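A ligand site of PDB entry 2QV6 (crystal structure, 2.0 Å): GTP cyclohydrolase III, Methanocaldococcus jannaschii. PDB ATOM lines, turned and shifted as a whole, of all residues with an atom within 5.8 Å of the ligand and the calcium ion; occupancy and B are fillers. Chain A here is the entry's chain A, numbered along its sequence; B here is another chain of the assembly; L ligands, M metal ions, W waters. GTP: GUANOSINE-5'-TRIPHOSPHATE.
The side-chain amino group (NZ) of Lys 213 is in salt-bridge range of an oxygen (O2G) of the ligand (3.5 Å).
The side-chain hydroxyl of Thr 143 sits at hydrogen-bond distance from an oxygen (O2B) of the ligand (2.6 Å).
An oxygen (O4') of the ligand sits close to the side-chain amide oxygen (OD1) of Asn 184 (3.2 Å).
The side-chain amide nitrogen (NE2) of Gln 112 of chain B sits at hydrogen-bond distance from an oxygen (O3A) of the ligand (3.1 Å).
The backbone NH of Asn 141 lies within hydrogen-bond range of an oxygen (O2G) of the ligand.
The side-chain carboxylate (OD2) of Asp 55 of chain B sits at hydrogen-bond distance from an oxygen (O3') of the ligand, at 2.6 Å.
The side-chain carboxylate (OE2) of Glu 24 of chain B lies within hydrogen-bond range of a nitrogen (N2) of the ligand (2.6 Å).
An oxygen (O1B) of the ligand sits close to the backbone NH of Ile 142.
OG1 of Thr 16 of chain B sits at hydrogen-bond distance from N7 of the ligand (3.2 Å).
N of Thr 143 is in hydrogen-bond range of O2B of the ligand (3.1 Å).
N2 of the ligand lies within hydrogen-bond range of O of Ile 180 (2.9 Å).
O1G of the ligand lies within salt-bridge range of NE of Arg 237 (2.7 Å).
NE2 of Gln 31 of chain B lies within hydrogen-bond range of OH of Tyr 12 of chain B, 2.6 Å away.
The side-chain hydroxyl (OG1) of Thr 143 is in hydrogen-bond range of the side-chain amide nitrogen (NE2) of Gln 112 of chain B (3.4 Å).
O of Ile 180 lies close to OE1 of Gln 28 of chain B, at 3.0 Å.
The side-chain amide oxygen (OE1) of Gln 28 of chain B lies close to the side-chain carboxylate (OE2) of Glu 24 of chain B, at 2.8 Å.
The side-chain hydroxyl (OG1) of Thr 16 of chain B lies within hydrogen-bond range of the backbone carbonyl oxygen (O) of Gly 13 of chain B.
The backbone carbonyl oxygen of Ile 180 lies close to the side-chain amide oxygen of Gln 31 of chain B (3.1 Å).
The side-chain carboxylate of Asp 138 sits close to the guanidinium group of Arg 237 (3.4 Å).
The guanidinium group (NH1) of Arg 53 of chain B lies within salt-bridge range of the side-chain carboxylate (OD1) of Asp 55 of chain B, 3.9 Å away.
CE1 of His 136 touches O6 of the ligand, 3.6 Å away.
CA of Asn 140 touches O2G of the ligand, 3.7 Å away.
Gly 181 touches the ligand.
Gly 182 touches the ligand (CA to O2', 3.5 Å).
Tyr 12 of chain B touches the ligand.
Gly 13 of chain B touches the ligand.
Leu 27 of chain B touches the ligand.
OE1 of Gln 28 of chain B touches N2 of the ligand (3.7 Å).
Of the 30 residues printed, 22 come within 4 Å of the ligand.
The nearest printed residue that does not touch the ligand is Asp 230 (4.1 Å).
Lys 213 touches the calcium ion.
Within 4 Å of the calcium ion: Asp 138, Ile 139, Asp 183 and Lys 213.
The nearest printed residue that does not touch the calcium ion is Arg 237 (4.04 Å).
The calcium ion is bound by O3G of the ligand, O of Ile 139, O1B of the ligand, OD1 of Asp 138, OD2 of Asp 183, OD2 of Asp 138 and O2A of the ligand.
The calcium ion has seven donor atoms within binding distance.
Water W4 bridges O1A of the ligand (2.6 Å) and O of Gly 13 of chain B (2.9 Å).
Water W1 lies within hydrogen-bond range of the side-chain amide nitrogen (NE2) of Gln 31 of chain B (2.7 Å) and an oxygen (O2') of the ligand (2.7 Å).
Water W2 lies within hydrogen-bond range of N of Gly 13 of chain B (3.0 Å), NE2 of Gln 112 of chain B (3.0 Å) and O3' of the ligand (3.0 Å).
Water W3 lies within hydrogen-bond range of the backbone carbonyl oxygen of Thr 16 of chain B, the backbone NH of Arg 22 of chain B and an oxygen (O6) of the ligand.
Water W5 lies within hydrogen-bond range of OD2 of Asp 55 of chain B (2.6 Å), ND2 of Asn 56 of chain B (3.3 Å) and O3' of the ligand (3.5 Å).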
ATOM      1  N   HIS A 136      18.444 -12.274  18.978  1.00  0.00           N
ATOM      2  CA  HIS A 136      17.835 -11.478  17.925  1.00  0.00           C
ATOM      3  C   HIS A 136      18.531 -11.904  16.633  1.00  0.00           C
ATOM      4  O   HIS A 136      19.684 -11.565  16.388  1.00  0.00           O
ATOM      5  CB  HIS A 136      18.060  -9.980  18.252  1.00  0.00           C
ATOM      6  CG  HIS A 136      17.353  -9.034  17.347  1.00  0.00           C
ATOM      7  ND1 HIS A 136      17.322  -7.670  17.579  1.00  0.00           N
ATOM      8  CD2 HIS A 136      16.644  -9.242  16.212  1.00  0.00           C
ATOM      9  CE1 HIS A 136      16.643  -7.088  16.617  1.00  0.00           C
ATOM     10  NE2 HIS A 136      16.196  -8.015  15.781  1.00  0.00           N
ATOM     11  N   ASP A 138      18.854 -12.363  12.436  1.00  0.00           N
ATOM     12  CA  ASP A 138      18.710 -11.459  11.313  1.00  0.00           C
ATOM     13  C   ASP A 138      19.433 -12.087  10.091  1.00  0.00           C
ATOM     14  O   ASP A 138      20.382 -12.819  10.254  1.00  0.00           O
ATOM     15  CB  ASP A 138      19.297 -10.070  11.712  1.00  0.00           C
ATOM     16  CG  ASP A 138      19.478  -9.109  10.532  1.00  0.00           C
ATOM     17  OD1 ASP A 138      18.477  -8.573  10.014  1.00  0.00           O
ATOM     18  OD2 ASP A 138      20.620  -8.852  10.117  1.00  0.00           O
ATOM     19  N   ILE A 139      18.975 -11.794   8.892  1.00  0.00           N
ATOM     20  CA  ILE A 139      19.615 -12.270   7.674  1.00  0.00           C
ATOM     21  C   ILE A 139      20.692 -11.264   7.198  1.00  0.00           C
ATOM     22  O   ILE A 139      20.521 -10.039   7.334  1.00  0.00           O
ATOM     23  CB  ILE A 139      18.526 -12.526   6.579  1.00  0.00           C
ATOM     24  CG1 ILE A 139      17.659 -13.723   7.003  1.00  0.00           C
ATOM     25  CG2 ILE A 139      19.160 -12.773   5.231  1.00  0.00           C
ATOM     26  CD1 ILE A 139      16.360 -13.868   6.261  1.00  0.00           C
ATOM     27  N   ASN A 140      21.825 -11.767   6.718  1.00  0.00           N
ATOM     28  CA  ASN A 140      22.919 -10.903   6.238  1.00  0.00           C
ATOM     29  C   ASN A 140      22.564 -10.433   4.856  1.00  0.00           C
ATOM     30  O   ASN A 140      22.260 -11.236   3.999  1.00  0.00           O
ATOM     31  CB  ASN A 140      24.268 -11.647   6.214  1.00  0.00           C
ATOM     32  CG  ASN A 140      24.884 -11.811   7.589  1.00  0.00           C
ATOM     33  OD1 ASN A 140      24.441 -11.196   8.558  1.00  0.00           O
ATOM     34  ND2 ASN A 140      25.913 -12.628   7.685  1.00  0.00           N
ATOM     35  N   ASN A 141      22.573  -9.133   4.659  1.00  0.00           N
ATOM     36  CA  ASN A 141      22.306  -8.527   3.364  1.00  0.00           C
ATOM     37  C   ASN A 141      21.018  -8.985   2.699  1.00  0.00           C
ATOM     38  O   ASN A 141      21.023  -9.366   1.518  1.00  0.00           O
ATOM     39  CB  ASN A 141      23.491  -8.728   2.413  1.00  0.00           C
ATOM     40  CG  ASN A 141      23.392  -7.863   1.158  1.00  0.00           C
ATOM     41  OD1 ASN A 141      22.723  -6.819   1.149  1.00  0.00           O
ATOM     42  ND2 ASN A 141      24.045  -8.308   0.076  1.00  0.00           N
ATOM     43  N   ILE A 142      19.897  -8.876   3.407  1.00  0.00           N
ATOM     44  CA  ILE A 142      18.576  -9.115   2.781  1.00  0.00           C
ATOM     45  C   ILE A 142      18.296  -8.144   1.614  1.00  0.00           C
ATOM     46  O   ILE A 142      17.640  -8.525   0.643  1.00  0.00           O
ATOM     47  CB  ILE A 142      17.386  -9.052   3.796  1.00  0.00           C
ATOM     48  CG1 ILE A 142      16.091  -9.626   3.178  1.00  0.00           C
ATOM     49  CG2 ILE A 142      17.110  -7.624   4.276  1.00  0.00           C
ATOM     50  CD1 ILE A 142      15.948 -11.090   3.304  1.00  0.00           C
ATOM     51  N   THR A 143      18.795  -6.920   1.682  1.00  0.00           N
ATOM     52  CA  THR A 143      18.390  -5.887   0.703  1.00  0.00           C
ATOM     53  C   THR A 143      19.042  -6.150  -0.646  1.00  0.00           C
ATOM     54  O   THR A 143      18.383  -6.073  -1.712  1.00  0.00           O
ATOM     55  CB  THR A 143      18.714  -4.462   1.205  1.00  0.00           C
ATOM     56  OG1 THR A 143      18.245  -4.299   2.534  1.00  0.00           O
ATOM     57  CG2 THR A 143      18.047  -3.404   0.314  1.00  0.00           C
ATOM     58  N   GLY A 144      20.330  -6.489  -0.612  1.00  0.00           N
ATOM     59  CA  GLY A 144      21.101  -6.743  -1.836  1.00  0.00           C
ATOM     60  C   GLY A 144      20.864  -8.107  -2.447  1.00  0.00           C
ATOM     61  O   GLY A 144      21.000  -8.265  -3.657  1.00  0.00           O
ATOM     62  N   ILE A 180       9.460 -10.662  13.838  1.00  0.00           N
ATOM     63  CA  ILE A 180       9.247  -9.284  14.310  1.00  0.00           C
ATOM     64  C   ILE A 180       9.297  -8.212  13.195  1.00  0.00           C
ATOM     65  O   ILE A 180       9.178  -7.011  13.460  1.00  0.00           O
ATOM     66  CB  ILE A 180      10.121  -8.968  15.580  1.00  0.00           C
ATOM     67  CG1 ILE A 180      11.597  -9.269  15.360  1.00  0.00           C
ATOM     68  CG2 ILE A 180       9.615  -9.824  16.737  1.00  0.00           C
ATOM     69  CD1 ILE A 180      12.563  -8.220  15.922  1.00  0.00           C
ATOM     70  N   GLY A 181       9.331  -8.661  11.952  1.00  0.00           N
ATOM     71  CA  GLY A 181       9.288  -7.787  10.796  1.00  0.00           C
ATOM     72  C   GLY A 181      10.618  -7.816  10.081  1.00  0.00           C
ATOM     73  O   GLY A 181      11.685  -8.094  10.690  1.00  0.00           O
ATOM     74  N   GLY A 182      10.562  -7.520   8.799  1.00  0.00           N
ATOM     75  CA  GLY A 182      11.735  -7.430   7.972  1.00  0.00           C
ATOM     76  C   GLY A 182      12.315  -8.785   7.642  1.00  0.00           C
ATOM     77  O   GLY A 182      11.689  -9.613   7.005  1.00  0.00           O
ATOM     78  N   ASP A 183      13.558  -8.983   8.079  1.00  0.00           N
ATOM     79  CA  ASP A 183      14.204 -10.269   8.025  1.00  0.00           C
ATOM     80  C   ASP A 183      14.603 -10.620   9.468  1.00  0.00           C
ATOM     81  O   ASP A 183      15.622 -11.239   9.677  1.00  0.00           O
ATOM     82  CB  ASP A 183      15.424 -10.199   7.102  1.00  0.00           C
ATOM     83  CG  ASP A 183      16.404  -9.091   7.465  1.00  0.00           C
ATOM     84  OD1 ASP A 183      15.980  -8.027   7.975  1.00  0.00           O
ATOM     85  OD2 ASP A 183      17.626  -9.248   7.242  1.00  0.00           O
ATOM     86  N   ASN A 184      13.781 -10.209  10.432  1.00  0.00           N
ATOM     87  CA  ASN A 184      14.122 -10.267  11.851  1.00  0.00           C
ATOM     88  C   ASN A 184      13.256 -11.250  12.614  1.00  0.00           C
ATOM     89  O   ASN A 184      12.069 -11.362  12.356  1.00  0.00           O
ATOM     90  CB  ASN A 184      13.999  -8.884  12.484  1.00  0.00           C
ATOM     91  CG  ASN A 184      15.143  -7.960  12.150  1.00  0.00           C
ATOM     92  OD1 ASN A 184      15.269  -7.488  11.020  1.00  0.00           O
ATOM     93  ND2 ASN A 184      15.966  -7.634  13.152  1.00  0.00           N
ATOM     94  N   LYS A 213      22.851 -14.108  11.414  1.00  0.00           N
ATOM     95  CA  LYS A 213      23.661 -13.670  12.548  1.00  0.00           C
ATOM     96  C   LYS A 213      22.742 -13.419  13.742  1.00  0.00           C
ATOM     97  O   LYS A 213      21.532 -13.331  13.594  1.00  0.00           O
ATOM     98  CB  LYS A 213      24.481 -12.420  12.181  1.00  0.00           C
ATOM     99  CG  LYS A 213      23.636 -11.279  11.610  1.00  0.00           C
ATOM    100  CD  LYS A 213      24.437  -9.971  11.457  1.00  0.00           C
ATOM    101  CE  LYS A 213      23.557  -8.804  10.977  1.00  0.00           C
ATOM    102  NZ  LYS A 213      23.027  -8.959   9.561  1.00  0.00           N
ATOM    103  N   ASP A 230      20.323  -6.275  20.797  1.00  0.00           N
ATOM    104  CA  ASP A 230      20.460  -5.284  19.713  1.00  0.00           C
ATOM    105  C   ASP A 230      21.896  -4.757  19.584  1.00  0.00           C
ATOM    106  O   ASP A 230      22.406  -4.557  18.480  1.00  0.00           O
ATOM    107  CB  ASP A 230      19.528  -4.084  19.934  1.00  0.00           C
ATOM    108  CG  ASP A 230      18.080  -4.360  19.566  1.00  0.00           C
ATOM    109  OD1 ASP A 230      17.781  -5.217  18.706  1.00  0.00           O
ATOM    110  OD2 ASP A 230      17.195  -3.687  20.129  1.00  0.00           O
ATOM    111  N   ARG A 237      27.891  -6.166  13.075  1.00  0.00           N
ATOM    112  CA  ARG A 237      27.930  -5.287  11.914  1.00  0.00           C
ATOM    113  C   ARG A 237      29.203  -4.448  11.817  1.00  0.00           C
ATOM    114  O   ARG A 237      29.731  -4.253  10.726  1.00  0.00           O
ATOM    115  CB  ARG A 237      26.731  -4.347  11.894  1.00  0.00           C
ATOM    116  CG  ARG A 237      25.456  -5.025  11.539  1.00  0.00           C
ATOM    117  CD  ARG A 237      24.445  -4.045  11.027  1.00  0.00           C
ATOM    118  NE  ARG A 237      23.245  -4.775  10.601  1.00  0.00           N
ATOM    119  CZ  ARG A 237      22.105  -4.826  11.274  1.00  0.00           C
ATOM    120  NH1 ARG A 237      21.947  -4.185  12.426  1.00  0.00           N
ATOM    121  NH2 ARG A 237      21.100  -5.530  10.781  1.00  0.00           N
ATOM    122  N   TYR B  12      14.202   2.161   5.890  1.00  0.00           N
ATOM    123  CA  TYR B  12      13.676   1.808   7.196  1.00  0.00           C
ATOM    124  C   TYR B  12      14.796   1.217   8.042  1.00  0.00           C
ATOM    125  O   TYR B  12      14.980   1.635   9.161  1.00  0.00           O
ATOM    126  CB  TYR B  12      12.468   0.866   7.058  1.00  0.00           C
ATOM    127  CG  TYR B  12      11.755   0.572   8.355  1.00  0.00           C
ATOM    128  CD1 TYR B  12      11.368   1.606   9.226  1.00  0.00           C
ATOM    129  CD2 TYR B  12      11.497  -0.743   8.750  1.00  0.00           C
ATOM    130  CE1 TYR B  12      10.722   1.327  10.447  1.00  0.00           C
ATOM    131  CE2 TYR B  12      10.864  -1.015   9.967  1.00  0.00           C
ATOM    132  CZ  TYR B  12      10.469   0.012  10.806  1.00  0.00           C
ATOM    133  OH  TYR B  12       9.859  -0.289  12.017  1.00  0.00           O
ATOM    134  N   GLY B  13      15.556   0.300   7.489  1.00  0.00           N
ATOM    135  CA  GLY B  13      16.655  -0.363   8.228  1.00  0.00           C
ATOM    136  C   GLY B  13      17.659   0.540   8.956  1.00  0.00           C
ATOM    137  O   GLY B  13      17.954   0.299  10.132  1.00  0.00           O
ATOM    138  N   PRO B  14      18.231   1.540   8.250  1.00  0.00           N
ATOM    139  CA  PRO B  14      19.066   2.553   8.913  1.00  0.00           C
ATOM    140  C   PRO B  14      18.386   3.417   9.983  1.00  0.00           C
ATOM    141  O   PRO B  14      19.041   3.809  10.945  1.00  0.00           O
ATOM    142  CB  PRO B  14      19.543   3.418   7.762  1.00  0.00           C
ATOM    143  CG  PRO B  14      19.482   2.523   6.562  1.00  0.00           C
ATOM    144  CD  PRO B  14      18.262   1.692   6.793  1.00  0.00           C
ATOM    145  N   THR B  16      16.077   2.462  12.150  1.00  0.00           N
ATOM    146  CA  THR B  16      15.865   1.656  13.366  1.00  0.00           C
ATOM    147  C   THR B  16      17.092   1.564  14.252  1.00  0.00           C
ATOM    148  O   THR B  16      16.987   1.127  15.403  1.00  0.00           O
ATOM    149  CB  THR B  16      15.414   0.188  13.042  1.00  0.00           C
ATOM    150  OG1 THR B  16      16.476  -0.526  12.395  1.00  0.00           O
ATOM    151  CG2 THR B  16      14.195   0.131  12.120  1.00  0.00           C
ATOM    152  N   VAL B  17      18.265   1.944  13.723  1.00  0.00           N
ATOM    153  CA  VAL B  17      19.546   1.886  14.454  1.00  0.00           C
ATOM    154  C   VAL B  17      20.337   3.208  14.490  1.00  0.00           C
ATOM    155  O   VAL B  17      21.422   3.282  15.095  1.00  0.00           O
ATOM    156  CB  VAL B  17      20.468   0.771  13.871  1.00  0.00           C
ATOM    157  CG1 VAL B  17      19.879  -0.632  14.138  1.00  0.00           C
ATOM    158  CG2 VAL B  17      20.689   0.990  12.381  1.00  0.00           C
ATOM    159  N   ARG B  22      16.545   0.852  18.893  1.00  0.00           N
ATOM    160  CA  ARG B  22      15.328   1.299  19.572  1.00  0.00           C
ATOM    161  C   ARG B  22      14.642   0.145  20.279  1.00  0.00           C
ATOM    162  O   ARG B  22      14.595  -0.935  19.736  1.00  0.00           O
ATOM    163  CB  ARG B  22      14.398   1.850  18.534  1.00  0.00           C
ATOM    164  CG  ARG B  22      15.001   2.973  17.714  1.00  0.00           C
ATOM    165  CD  ARG B  22      14.058   3.496  16.688  1.00  0.00           C
ATOM    166  NE  ARG B  22      14.738   4.410  15.775  1.00  0.00           N
ATOM    167  CZ  ARG B  22      14.889   5.729  15.954  1.00  0.00           C
ATOM    168  NH1 ARG B  22      14.385   6.349  17.000  1.00  0.00           N
ATOM    169  NH2 ARG B  22      15.535   6.444  15.039  1.00  0.00           N
ATOM    170  N   GLU B  24      12.403  -2.682  21.272  1.00  0.00           N
ATOM    171  CA  GLU B  24      11.615  -3.497  20.355  1.00  0.00           C
ATOM    172  C   GLU B  24      10.095  -3.391  20.555  1.00  0.00           C
ATOM    173  O   GLU B  24       9.360  -3.367  19.572  1.00  0.00           O
ATOM    174  CB  GLU B  24      12.052  -4.964  20.423  1.00  0.00           C
ATOM    175  CG  GLU B  24      11.491  -5.861  19.320  1.00  0.00           C
ATOM    176  CD  GLU B  24      11.798  -5.359  17.904  1.00  0.00           C
ATOM    177  OE1 GLU B  24      12.934  -4.907  17.611  1.00  0.00           O
ATOM    178  OE2 GLU B  24      10.888  -5.423  17.056  1.00  0.00           O
ATOM    179  N   LEU B  27       8.917  -0.617  18.540  1.00  0.00           N
ATOM    180  CA  LEU B  27       8.946  -0.930  17.112  1.00  0.00           C
ATOM    181  C   LEU B  27       7.762  -1.792  16.719  1.00  0.00           C
ATOM    182  O   LEU B  27       7.208  -1.632  15.630  1.00  0.00           O
ATOM    183  CB  LEU B  27      10.267  -1.602  16.698  1.00  0.00           C
ATOM    184  CG  LEU B  27      11.526  -0.707  16.631  1.00  0.00           C
ATOM    185  CD1 LEU B  27      12.678  -1.497  16.082  1.00  0.00           C
ATOM    186  CD2 LEU B  27      11.340   0.563  15.798  1.00  0.00           C
ATOM    187  N   GLN B  28       7.336  -2.672  17.628  1.00  0.00           N
ATOM    188  CA  GLN B  28       6.151  -3.490  17.403  1.00  0.00           C
ATOM    189  C   GLN B  28       4.856  -2.688  17.389  1.00  0.00           C
ATOM    190  O   GLN B  28       4.011  -2.886  16.493  1.00  0.00           O
ATOM    191  CB  GLN B  28       6.068  -4.642  18.415  1.00  0.00           C
ATOM    192  CG  GLN B  28       7.200  -5.604  18.259  1.00  0.00           C
ATOM    193  CD  GLN B  28       7.273  -6.227  16.881  1.00  0.00           C
ATOM    194  OE1 GLN B  28       8.287  -6.114  16.181  1.00  0.00           O
ATOM    195  NE2 GLN B  28       6.225  -6.913  16.492  1.00  0.00           N
ATOM    196  N   GLN B  31       4.926  -0.498  14.119  1.00  0.00           N
ATOM    197  CA  GLN B  31       4.649  -1.291  12.899  1.00  0.00           C
ATOM    198  C   GLN B  31       3.194  -1.724  12.752  1.00  0.00           C
ATOM    199  O   GLN B  31       2.615  -1.669  11.630  1.00  0.00           O
ATOM    200  CB  GLN B  31       5.606  -2.496  12.812  1.00  0.00           C
ATOM    201  CG  GLN B  31       6.969  -2.121  12.223  1.00  0.00           C
ATOM    202  CD  GLN B  31       8.072  -3.157  12.440  1.00  0.00           C
ATOM    203  OE1 GLN B  31       7.806  -4.290  12.809  1.00  0.00           O
ATOM    204  NE2 GLN B  31       9.282  -2.781  12.152  1.00  0.00           N
ATOM    205  N   ARG B  53       5.557  -8.445   5.394  1.00  0.00           N
ATOM    206  CA  ARG B  53       6.774  -8.343   6.246  1.00  0.00           C
ATOM    207  C   ARG B  53       6.853  -7.102   7.147  1.00  0.00           C
ATOM    208  O   ARG B  53       7.880  -6.876   7.824  1.00  0.00           O
ATOM    209  CB  ARG B  53       8.032  -8.425   5.386  1.00  0.00           C
ATOM    210  CG  ARG B  53       8.030  -9.648   4.485  1.00  0.00           C
ATOM    211  CD  ARG B  53       9.416 -10.035   4.042  1.00  0.00           C
ATOM    212  NE  ARG B  53       9.950  -9.091   3.060  1.00  0.00           N
ATOM    213  CZ  ARG B  53      11.045  -8.347   3.245  1.00  0.00           C
ATOM    214  NH1 ARG B  53      11.795  -8.466   4.349  1.00  0.00           N
ATOM    215  NH2 ARG B  53      11.432  -7.527   2.298  1.00  0.00           N
ATOM    216  N   ASP B  55       7.690  -4.045   7.104  1.00  0.00           N
ATOM    217  CA  ASP B  55       8.387  -3.017   6.309  1.00  0.00           C
ATOM    218  C   ASP B  55       8.026  -3.032   4.806  1.00  0.00           C
ATOM    219  O   ASP B  55       8.344  -2.078   4.113  1.00  0.00           O
ATOM    220  CB  ASP B  55       9.903  -3.087   6.447  1.00  0.00           C
ATOM    221  CG  ASP B  55      10.535  -4.291   5.726  1.00  0.00           C
ATOM    222  OD1 ASP B  55       9.895  -5.354   5.636  1.00  0.00           O
ATOM    223  OD2 ASP B  55      11.685  -4.179   5.231  1.00  0.00           O
ATOM    224  N   ASN B  56       7.409  -4.124   4.325  1.00  0.00           N
ATOM    225  CA  ASN B  56       6.850  -4.240   2.943  1.00  0.00           C
ATOM    226  C   ASN B  56       5.437  -4.824   3.015  1.00  0.00           C
ATOM    227  O   ASN B  56       5.271  -5.865   3.626  1.00  0.00           O
ATOM    228  CB  ASN B  56       7.697  -5.200   2.077  1.00  0.00           C
ATOM    229  CG  ASN B  56       9.014  -4.606   1.590  1.00  0.00           C
ATOM    230  OD1 ASN B  56       9.085  -4.087   0.485  1.00  0.00           O
ATOM    231  ND2 ASN B  56      10.056  -4.697   2.397  1.00  0.00           N
ATOM    232  N   GLN B 112      17.150   0.857   0.659  1.00  0.00           N
ATOM    233  CA  GLN B 112      17.972   1.595   1.635  1.00  0.00           C
ATOM    234  C   GLN B 112      18.806   2.679   0.954  1.00  0.00           C
ATOM    235  O   GLN B 112      20.002   2.781   1.148  1.00  0.00           O
ATOM    236  CB  GLN B 112      18.836   0.605   2.420  1.00  0.00           C
ATOM    237  CG  GLN B 112      18.009  -0.393   3.218  1.00  0.00           C
ATOM    238  CD  GLN B 112      18.827  -1.189   4.202  1.00  0.00           C
ATOM    239  OE1 GLN B 112      20.039  -1.073   4.245  1.00  0.00           O
ATOM    240  NE2 GLN B 112      18.153  -2.014   4.995  1.00  0.00           N
HETATM  241  PG  GTP L   1      22.539  -6.158   7.224  1.00  0.00           P
HETATM  242  O1G GTP L   1      23.374  -5.138   7.947  1.00  0.00           O
HETATM  243  O2G GTP L   1      23.358  -7.225   6.577  1.00  0.00           O
HETATM  244  O3G GTP L   1      21.527  -6.896   8.020  1.00  0.00           O
HETATM  245  O3B GTP L   1      21.771  -5.335   6.039  1.00  0.00           O
HETATM  246  PB  GTP L   1      20.313  -5.739   5.571  1.00  0.00           P
HETATM  247  O1B GTP L   1      19.865  -7.119   5.955  1.00  0.00           O
HETATM  248  O2B GTP L   1      20.009  -5.427   4.085  1.00  0.00           O
HETATM  249  O3A GTP L   1      19.228  -4.677   6.143  1.00  0.00           O
HETATM  250  PA  GTP L   1      18.611  -4.547   7.606  1.00  0.00           P
HETATM  251  O1A GTP L   1      19.386  -3.479   8.367  1.00  0.00           O
HETATM  252  O2A GTP L   1      18.598  -5.845   8.372  1.00  0.00           O
HETATM  253  O5' GTP L   1      17.134  -4.023   7.386  1.00  0.00           O
HETATM  254  C5' GTP L   1      16.173  -4.762   6.694  1.00  0.00           C
HETATM  255  C4' GTP L   1      14.899  -4.717   7.543  1.00  0.00           C
HETATM  256  O4' GTP L   1      15.149  -5.172   8.878  1.00  0.00           O
HETATM  257  C3' GTP L   1      14.301  -3.348   7.726  1.00  0.00           C
HETATM  258  O3' GTP L   1      13.501  -2.971   6.611  1.00  0.00           O
HETATM  259  C2' GTP L   1      13.474  -3.549   8.962  1.00  0.00           C
HETATM  260  O2' GTP L   1      12.223  -4.043   8.554  1.00  0.00           O
HETATM  261  C1' GTP L   1      14.147  -4.656   9.738  1.00  0.00           C
HETATM  262  N9  GTP L   1      14.765  -4.302  11.038  1.00  0.00           N
HETATM  263  C8  GTP L   1      16.032  -3.803  11.258  1.00  0.00           C
HETATM  264  N7  GTP L   1      16.232  -3.707  12.597  1.00  0.00           N
HETATM  265  C5  GTP L   1      15.115  -4.140  13.213  1.00  0.00           C
HETATM  266  C6  GTP L   1      14.807  -4.238  14.544  1.00  0.00           C
HETATM  267  O6  GTP L   1      15.578  -3.893  15.485  1.00  0.00           O
HETATM  268  N1  GTP L   1      13.583  -4.748  14.879  1.00  0.00           N
HETATM  269  C2  GTP L   1      12.660  -5.131  13.959  1.00  0.00           C
HETATM  270  N2  GTP L   1      11.529  -5.587  14.498  1.00  0.00           N
HETATM  271  N3  GTP L   1      12.924  -5.048  12.600  1.00  0.00           N
HETATM  272  C4  GTP L   1      14.184  -4.559  12.256  1.00  0.00           C
HETATM  273 CA    CA M   1      19.642  -8.070   7.995  1.00  0.00          CA
HETATM  274  O   HOH W   1      10.748  -4.564  10.789  1.00  0.00           O
HETATM  275  O   HOH W   2      15.279  -1.234   4.969  1.00  0.00           O
HETATM  276  O   HOH W   3      16.762  -1.267  16.723  1.00  0.00           O
HETATM  277  O   HOH W   4      19.266  -2.246  10.622  1.00  0.00           O
HETATM  278  O   HOH W   5      12.731  -2.988   3.233  1.00  0.00           O
